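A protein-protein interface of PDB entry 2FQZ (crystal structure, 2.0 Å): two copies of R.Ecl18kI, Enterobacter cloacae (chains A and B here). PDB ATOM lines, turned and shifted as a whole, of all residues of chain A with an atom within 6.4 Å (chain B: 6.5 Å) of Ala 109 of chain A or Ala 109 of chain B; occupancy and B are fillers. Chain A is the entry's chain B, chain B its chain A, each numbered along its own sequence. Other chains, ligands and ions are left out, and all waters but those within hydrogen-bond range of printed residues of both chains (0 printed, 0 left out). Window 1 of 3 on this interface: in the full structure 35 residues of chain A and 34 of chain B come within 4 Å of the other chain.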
ATOM      1  N   ILE A  13      -3.772 -18.990  39.233  1.00  0.00           N
ATOM      2  CA  ILE A  13      -3.148 -17.674  39.072  1.00  0.00           C
ATOM      3  C   ILE A  13      -3.473 -16.825  40.295  1.00  0.00           C
ATOM      4  O   ILE A  13      -2.585 -16.222  40.888  1.00  0.00           O
ATOM      5  CB  ILE A  13      -3.603 -16.943  37.785  1.00  0.00           C
ATOM      6  CG1 ILE A  13      -3.171 -17.704  36.535  1.00  0.00           C
ATOM      7  CG2 ILE A  13      -3.016 -15.526  37.731  1.00  0.00           C
ATOM      8  CD1 ILE A  13      -4.001 -17.385  35.322  1.00  0.00           C
ATOM      9  N   THR A  72       4.608 -14.508  35.357  1.00  0.00           N
ATOM     10  CA  THR A  72       3.881 -14.839  34.144  1.00  0.00           C
ATOM     11  C   THR A  72       4.523 -16.062  33.479  1.00  0.00           C
ATOM     12  O   THR A  72       3.836 -17.034  33.134  1.00  0.00           O
ATOM     13  CB  THR A  72       3.863 -13.662  33.158  1.00  0.00           C
ATOM     14  OG1 THR A  72       3.274 -12.520  33.793  1.00  0.00           O
ATOM     15  CG2 THR A  72       3.031 -14.018  31.911  1.00  0.00           C
ATOM     16  N   HIS A 104      -6.272 -19.893  28.527  1.00  0.00           N
ATOM     17  CA  HIS A 104      -5.330 -19.878  29.644  1.00  0.00           C
ATOM     18  C   HIS A 104      -4.409 -18.675  29.554  1.00  0.00           C
ATOM     19  O   HIS A 104      -4.362 -17.858  30.480  1.00  0.00           O
ATOM     20  CB  HIS A 104      -4.489 -21.146  29.653  1.00  0.00           C
ATOM     21  CG  HIS A 104      -5.296 -22.396  29.618  1.00  0.00           C
ATOM     22  ND1 HIS A 104      -5.913 -22.849  28.472  1.00  0.00           N
ATOM     23  CD2 HIS A 104      -5.577 -23.302  30.583  1.00  0.00           C
ATOM     24  CE1 HIS A 104      -6.536 -23.982  28.731  1.00  0.00           C
ATOM     25  NE2 HIS A 104      -6.347 -24.281  30.004  1.00  0.00           N
ATOM     26  N   ILE A 105      -3.697 -18.574  28.426  1.00  0.00           N
ATOM     27  CA  ILE A 105      -2.762 -17.483  28.163  1.00  0.00           C
ATOM     28  C   ILE A 105      -3.451 -16.120  28.331  1.00  0.00           C
ATOM     29  O   ILE A 105      -2.957 -15.249  29.055  1.00  0.00           O
ATOM     30  CB  ILE A 105      -2.144 -17.584  26.749  1.00  0.00           C
ATOM     31  CG1 ILE A 105      -1.257 -18.835  26.627  1.00  0.00           C
ATOM     32  CG2 ILE A 105      -1.311 -16.340  26.441  1.00  0.00           C
ATOM     33  CD1 ILE A 105      -0.647 -19.022  25.249  1.00  0.00           C
ATOM     34  N   TYR A 106      -4.577 -15.954  27.642  1.00  0.00           N
ATOM     35  CA  TYR A 106      -5.389 -14.757  27.743  1.00  0.00           C
ATOM     36  C   TYR A 106      -5.880 -14.500  29.176  1.00  0.00           C
ATOM     37  O   TYR A 106      -5.793 -13.364  29.652  1.00  0.00           O
ATOM     38  CB  TYR A 106      -6.561 -14.784  26.737  1.00  0.00           C
ATOM     39  CG  TYR A 106      -7.538 -13.656  26.989  1.00  0.00           C
ATOM     40  CD1 TYR A 106      -7.295 -12.376  26.497  1.00  0.00           C
ATOM     41  CD2 TYR A 106      -8.684 -13.861  27.756  1.00  0.00           C
ATOM     42  CE1 TYR A 106      -8.183 -11.331  26.751  1.00  0.00           C
ATOM     43  CE2 TYR A 106      -9.558 -12.820  28.027  1.00  0.00           C
ATOM     44  CZ  TYR A 106      -9.305 -11.570  27.513  1.00  0.00           C
ATOM     45  OH  TYR A 106     -10.182 -10.540  27.775  1.00  0.00           O
ATOM     46  N   ASP A 107      -6.386 -15.526  29.865  1.00  0.00           N
ATOM     47  CA  ASP A 107      -6.881 -15.342  31.244  1.00  0.00           C
ATOM     48  C   ASP A 107      -5.780 -14.870  32.167  1.00  0.00           C
ATOM     49  O   ASP A 107      -6.018 -14.067  33.071  1.00  0.00           O
ATOM     50  CB  ASP A 107      -7.466 -16.627  31.831  1.00  0.00           C
ATOM     51  CG  ASP A 107      -8.770 -17.015  31.188  1.00  0.00           C
ATOM     52  OD1 ASP A 107      -9.316 -16.183  30.442  1.00  0.00           O
ATOM     53  OD2 ASP A 107      -9.229 -18.161  31.401  1.00  0.00           O
ATOM     54  N   LEU A 108      -4.586 -15.404  31.951  1.00  0.00           N
ATOM     55  CA  LEU A 108      -3.421 -15.003  32.717  1.00  0.00           C
ATOM     56  C   LEU A 108      -3.083 -13.538  32.478  1.00  0.00           C
ATOM     57  O   LEU A 108      -2.912 -12.780  33.433  1.00  0.00           O
ATOM     58  CB  LEU A 108      -2.222 -15.890  32.370  1.00  0.00           C
ATOM     59  CG  LEU A 108      -0.838 -15.381  32.799  1.00  0.00           C
ATOM     60  CD1 LEU A 108      -0.737 -15.119  34.302  1.00  0.00           C
ATOM     61  CD2 LEU A 108       0.201 -16.380  32.352  1.00  0.00           C
ATOM     62  N   ALA A 109      -2.979 -13.146  31.210  1.00  0.00           N
ATOM     63  CA  ALA A 109      -2.690 -11.758  30.873  1.00  0.00           C
ATOM     64  C   ALA A 109      -3.813 -10.825  31.341  1.00  0.00           C
ATOM     65  O   ALA A 109      -3.546  -9.680  31.763  1.00  0.00           O
ATOM     66  CB  ALA A 109      -2.439 -11.619  29.391  1.00  0.00           C
ATOM     67  N   LEU A 110      -5.054 -11.323  31.281  1.00  0.00           N
ATOM     68  CA  LEU A 110      -6.213 -10.610  31.817  1.00  0.00           C
ATOM     69  C   LEU A 110      -6.081 -10.418  33.326  1.00  0.00           C
ATOM     70  O   LEU A 110      -6.303  -9.324  33.833  1.00  0.00           O
ATOM     71  CB  LEU A 110      -7.553 -11.299  31.482  1.00  0.00           C
ATOM     72  CG  LEU A 110      -8.827 -10.608  32.018  1.00  0.00           C
ATOM     73  CD1 LEU A 110      -8.913  -9.153  31.586  1.00  0.00           C
ATOM     74  CD2 LEU A 110     -10.094 -11.334  31.619  1.00  0.00           C
ATOM     75  N   SER A 111      -5.723 -11.486  34.033  1.00  0.00           N
ATOM     76  CA  SER A 111      -5.552 -11.399  35.474  1.00  0.00           C
ATOM     77  C   SER A 111      -4.426 -10.432  35.813  1.00  0.00           C
ATOM     78  O   SER A 111      -4.556  -9.656  36.746  1.00  0.00           O
ATOM     79  CB  SER A 111      -5.270 -12.764  36.083  1.00  0.00           C
ATOM     80  OG  SER A 111      -5.220 -12.642  37.493  1.00  0.00           O
ATOM     81  N   ASN A 112      -3.338 -10.493  35.043  1.00  0.00           N
ATOM     82  CA  ASN A 112      -2.219  -9.550  35.142  1.00  0.00           C
ATOM     83  C   ASN A 112      -2.635  -8.083  34.977  1.00  0.00           C
ATOM     84  O   ASN A 112      -2.339  -7.255  35.855  1.00  0.00           O
ATOM     85  CB  ASN A 112      -1.138  -9.879  34.111  1.00  0.00           C
ATOM     86  CG  ASN A 112      -0.248 -11.036  34.527  1.00  0.00           C
ATOM     87  OD1 ASN A 112      -0.482 -11.712  35.534  1.00  0.00           O
ATOM     88  ND2 ASN A 112       0.791 -11.264  33.740  1.00  0.00           N
ATOM     89  N   THR A 113      -3.323  -7.748  33.880  1.00  0.00           N
ATOM     90  CA  THR A 113      -3.745  -6.351  33.697  1.00  0.00           C
ATOM     91  C   THR A 113      -4.723  -5.857  34.766  1.00  0.00           C
ATOM     92  O   THR A 113      -4.664  -4.710  35.187  1.00  0.00           O
ATOM     93  CB  THR A 113      -4.223  -5.999  32.260  1.00  0.00           C
ATOM     94  OG1 THR A 113      -4.306  -4.566  32.139  1.00  0.00           O
ATOM     95  CG2 THR A 113      -5.580  -6.639  31.929  1.00  0.00           C
ATOM     96  N   GLN A 114      -5.586  -6.744  35.236  1.00  0.00           N
ATOM     97  CA  GLN A 114      -6.585  -6.368  36.212  1.00  0.00           C
ATOM     98  C   GLN A 114      -5.918  -6.125  37.550  1.00  0.00           C
ATOM     99  O   GLN A 114      -6.317  -5.224  38.299  1.00  0.00           O
ATOM    100  CB  GLN A 114      -7.650  -7.448  36.309  1.00  0.00           C
ATOM    101  CG  GLN A 114      -8.450  -7.636  35.008  1.00  0.00           C
ATOM    102  CD  GLN A 114      -9.407  -6.490  34.717  1.00  0.00           C
ATOM    103  OE1 GLN A 114      -8.993  -5.375  34.411  1.00  0.00           O
ATOM    104  NE2 GLN A 114     -10.689  -6.764  34.803  1.00  0.00           N
ATOM    105  N   THR B  72      -5.471 -14.597  17.866  1.00  0.00           N
ATOM    106  CA  THR B  72      -4.401 -14.538  18.843  1.00  0.00           C
ATOM    107  C   THR B  72      -3.290 -15.490  18.388  1.00  0.00           C
ATOM    108  O   THR B  72      -2.103 -15.132  18.323  1.00  0.00           O
ATOM    109  CB  THR B  72      -4.957 -14.972  20.211  1.00  0.00           C
ATOM    110  OG1 THR B  72      -6.021 -14.081  20.589  1.00  0.00           O
ATOM    111  CG2 THR B  72      -3.864 -14.980  21.290  1.00  0.00           C
ATOM    112  N   HIS B 104       5.378  -9.407  24.645  1.00  0.00           N
ATOM    113  CA  HIS B 104       4.668  -9.630  23.380  1.00  0.00           C
ATOM    114  C   HIS B 104       3.348 -10.368  23.619  1.00  0.00           C
ATOM    115  O   HIS B 104       2.328 -10.001  23.038  1.00  0.00           O
ATOM    116  CB  HIS B 104       5.536 -10.444  22.399  1.00  0.00           C
ATOM    117  CG  HIS B 104       6.773  -9.737  21.931  1.00  0.00           C
ATOM    118  ND1 HIS B 104       7.948  -9.724  22.654  1.00  0.00           N
ATOM    119  CD2 HIS B 104       7.024  -9.040  20.796  1.00  0.00           C
ATOM    120  CE1 HIS B 104       8.863  -9.037  21.990  1.00  0.00           C
ATOM    121  NE2 HIS B 104       8.328  -8.612  20.859  1.00  0.00           N
ATOM    122  N   ILE B 105       3.376 -11.397  24.474  1.00  0.00           N
ATOM    123  CA  ILE B 105       2.186 -12.194  24.797  1.00  0.00           C
ATOM    124  C   ILE B 105       1.191 -11.401  25.642  1.00  0.00           C
ATOM    125  O   ILE B 105      -0.018 -11.489  25.421  1.00  0.00           O
ATOM    126  CB  ILE B 105       2.553 -13.503  25.523  1.00  0.00           C
ATOM    127  CG1 ILE B 105       3.323 -14.449  24.575  1.00  0.00           C
ATOM    128  CG2 ILE B 105       1.323 -14.202  26.074  1.00  0.00           C
ATOM    129  CD1 ILE B 105       4.029 -15.559  25.294  1.00  0.00           C
ATOM    130  N   TYR B 106       1.712 -10.661  26.622  1.00  0.00           N
ATOM    131  CA  TYR B 106       0.866  -9.774  27.415  1.00  0.00           C
ATOM    132  C   TYR B 106       0.268  -8.695  26.523  1.00  0.00           C
ATOM    133  O   TYR B 106      -0.933  -8.461  26.576  1.00  0.00           O
ATOM    134  CB  TYR B 106       1.638  -9.158  28.587  1.00  0.00           C
ATOM    135  CG  TYR B 106       0.824  -8.159  29.378  1.00  0.00           C
ATOM    136  CD1 TYR B 106      -0.224  -8.582  30.199  1.00  0.00           C
ATOM    137  CD2 TYR B 106       1.092  -6.798  29.294  1.00  0.00           C
ATOM    138  CE1 TYR B 106      -0.985  -7.659  30.929  1.00  0.00           C
ATOM    139  CE2 TYR B 106       0.341  -5.872  30.020  1.00  0.00           C
ATOM    140  CZ  TYR B 106      -0.689  -6.314  30.831  1.00  0.00           C
ATOM    141  OH  TYR B 106      -1.431  -5.405  31.555  1.00  0.00           O
ATOM    142  N   ASP B 107       1.098  -8.043  25.711  1.00  0.00           N
ATOM    143  CA  ASP B 107       0.637  -6.980  24.819  1.00  0.00           C
ATOM    144  C   ASP B 107      -0.483  -7.385  23.880  1.00  0.00           C
ATOM    145  O   ASP B 107      -1.336  -6.558  23.535  1.00  0.00           O
ATOM    146  CB  ASP B 107       1.783  -6.370  24.019  1.00  0.00           C
ATOM    147  CG  ASP B 107       2.609  -5.390  24.834  1.00  0.00           C
ATOM    148  OD1 ASP B 107       2.286  -5.173  26.023  1.00  0.00           O
ATOM    149  OD2 ASP B 107       3.580  -4.834  24.279  1.00  0.00           O
ATOM    150  N   LEU B 108      -0.478  -8.649  23.468  1.00  0.00           N
ATOM    151  CA  LEU B 108      -1.522  -9.177  22.615  1.00  0.00           C
ATOM    152  C   LEU B 108      -2.798  -9.486  23.400  1.00  0.00           C
ATOM    153  O   LEU B 108      -3.895  -9.163  22.938  1.00  0.00           O
ATOM    154  CB  LEU B 108      -1.023 -10.419  21.847  1.00  0.00           C
ATOM    155  CG  LEU B 108      -2.084 -11.341  21.234  1.00  0.00           C
ATOM    156  CD1 LEU B 108      -3.015 -10.645  20.246  1.00  0.00           C
ATOM    157  CD2 LEU B 108      -1.392 -12.499  20.557  1.00  0.00           C
ATOM    158  N   ALA B 109      -2.664 -10.102  24.573  1.00  0.00           N
ATOM    159  CA  ALA B 109      -3.858 -10.403  25.369  1.00  0.00           C
ATOM    160  C   ALA B 109      -4.445  -9.127  25.985  1.00  0.00           C
ATOM    161  O   ALA B 109      -5.658  -9.046  26.195  1.00  0.00           O
ATOM    162  CB  ALA B 109      -3.556 -11.415  26.430  1.00  0.00           C
ATOM    163  N   LEU B 110      -3.586  -8.141  26.245  1.00  0.00           N
ATOM    164  CA  LEU B 110      -4.039  -6.826  26.715  1.00  0.00           C
ATOM    165  C   LEU B 110      -4.873  -6.141  25.625  1.00  0.00           C
ATOM    166  O   LEU B 110      -5.976  -5.645  25.885  1.00  0.00           O
ATOM    167  CB  LEU B 110      -2.846  -5.946  27.120  1.00  0.00           C
ATOM    168  CG  LEU B 110      -3.173  -4.500  27.544  1.00  0.00           C
ATOM    169  CD1 LEU B 110      -4.263  -4.521  28.594  1.00  0.00           C
ATOM    170  CD2 LEU B 110      -1.942  -3.766  28.026  1.00  0.00           C
ATOM    171  N   SER B 111      -4.333  -6.135  24.405  1.00  0.00           N
ATOM    172  CA  SER B 111      -4.991  -5.548  23.246  1.00  0.00           C
ATOM    173  C   SER B 111      -6.353  -6.194  23.042  1.00  0.00           C
ATOM    174  O   SER B 111      -7.349  -5.509  22.771  1.00  0.00           O
ATOM    175  CB  SER B 111      -4.135  -5.740  21.996  1.00  0.00           C
ATOM    176  OG  SER B 111      -4.485  -4.803  20.988  1.00  0.00           O
ATOM    177  N   ASN B 112      -6.389  -7.515  23.193  1.00  0.00           N
ATOM    178  CA  ASN B 112      -7.635  -8.267  23.099  1.00  0.00           C
ATOM    179  C   ASN B 112      -8.701  -7.897  24.118  1.00  0.00           C
ATOM    180  O   ASN B 112      -9.859  -7.710  23.754  1.00  0.00           O
ATOM    181  CB  ASN B 112      -7.365  -9.759  23.200  1.00  0.00           C
ATOM    182  CG  ASN B 112      -6.774 -10.323  21.936  1.00  0.00           C
ATOM    183  OD1 ASN B 112      -6.701  -9.646  20.904  1.00  0.00           O
ATOM    184  ND2 ASN B 112      -6.350 -11.576  22.007  1.00  0.00           N
ATOM    185  N   THR B 113      -8.332  -7.855  25.391  1.00  0.00           N
ATOM    186  CA  THR B 113      -9.301  -7.487  26.424  1.00  0.00           C
ATOM    187  C   THR B 113      -9.754  -6.040  26.232  1.00  0.00           C
ATOM    188  O   THR B 113     -10.923  -5.716  26.466  1.00  0.00           O
ATOM    189  CB  THR B 113      -8.800  -7.745  27.881  1.00  0.00           C
ATOM    190  OG1 THR B 113      -9.875  -7.532  28.800  1.00  0.00           O
ATOM    191  CG2 THR B 113      -7.658  -6.846  28.264  1.00  0.00           C
ATOM    192  N   GLN B 114      -8.848  -5.184  25.771  1.00  0.00           N
ATOM    193  CA  GLN B 114      -9.202  -3.794  25.502  1.00  0.00           C
ATOM    194  C   GLN B 114     -10.195  -3.679  24.351  1.00  0.00           C
ATOM    195  O   GLN B 114     -11.122  -2.867  24.399  1.00  0.00           O
ATOM    196  CB  GLN B 114      -7.946  -2.945  25.286  1.00  0.00           C
ATOM    197  CG  GLN B 114      -7.062  -2.888  26.517  1.00  0.00           C
ATOM    198  CD  GLN B 114      -7.658  -2.051  27.647  1.00  0.00           C
ATOM    199  OE1 GLN B 114      -8.677  -2.404  28.245  1.00  0.00           O
ATOM    200  NE2 GLN B 114      -7.020  -0.952  27.928  1.00  0.00           N
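Ile 105 of chain B touches its own counterpart, Ile 105 of chain A. Tyr 106 of chain A touches Ala 109 of chain B, and with the chains exchanged Ala 109 of chain A touches Tyr 106 of chain B. Tyr 106 of chain A touches Thr 113 of chain B, and with the chains exchanged Thr 113 of chain A touches Tyr 106 of chain B. Leu 110 of chain A touches Thr 113 of chain B, and with the chains exchanged Thr 113 of chain A touches Leu 110 of chain B.
Ala 109 of chain A touches two residues of chain B. Of chain A, only Tyr 106 (3.5 Å) and Ala 109 (3.2 Å) come within 4 Å of Ala 109 of chain B. Of the printed residues of chain B, Thr 113 of chain A touches Tyr 106 and Leu 110. Of the printed residues of chain A, Ile 105 of chain B touches Ile 105 (3.4 Å). Printed residues of chain A within 4 Å of Tyr 106 of chain B: Ala 109, Asn 112 and Thr 113. Of the printed residues of chain B, Leu 110 of chain A touches Thr 113 (3.4 Å). Of the printed residues of chain A, Asn 112 of chain B touches Tyr 106. Leu 108 of chain A touches none of the printed residues of chain B. Gln 114 of chain B touches none of the printed residues of chain A. The nearest residue of chain B that does not touch Ala 109 of chain A is Ile 105 of chain B (4.7 Å).
The side-chain hydroxyl (OG1) of Thr 72 of chain B sits at hydrogen-bond distance from the side-chain amide nitrogen (ND2) of Asn 112 of chain B, at 2.9 Å. OD1 of Asn 112 of chain B sits close to O of Leu 108 of chain B. The side-chain hydroxyl (OG1) of Thr 72 of chain A is in hydrogen-bond range of the side-chain amide nitrogen (ND2) of Asn 112 of chain A (2.8 Å). The side-chain amide oxygen (OD1) of Asn 112 of chain A lies close to the backbone carbonyl oxygen (O) of Leu 108 of chain A.
OG1 of Thr 113 of chain A lies close to OH of Tyr 106 of chain B (3.1 Å). OH of Tyr 106 of chain A lies close to OG1 of Thr 113 of chain B (3.2 Å).
Among the printed residues, merely in contact across the chains: Ile 105 of chain A with Ile 105 of chain B, Tyr 106 of chain A with Ala 109 of chain B, Tyr 106 of chain A with Asn 112 of chain B, Ala 109 of chain A with Tyr 106 of chain B, Ala 109 of chain A with Ala 109 of chain B, Leu 110 of chain A with Thr 113 of chain B, Asn 112 of chain A with Tyr 106 of chain B and Thr 113 of chain A with Leu 110 of chain B.
Hydrophobic or aromatic side chains of chain A that line the printed part of chain B: Ile 105, Tyr 106, Ala 109 and Leu 110. Of the 12 printed residues of chain B, 6 touch a printed residue of chain A.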
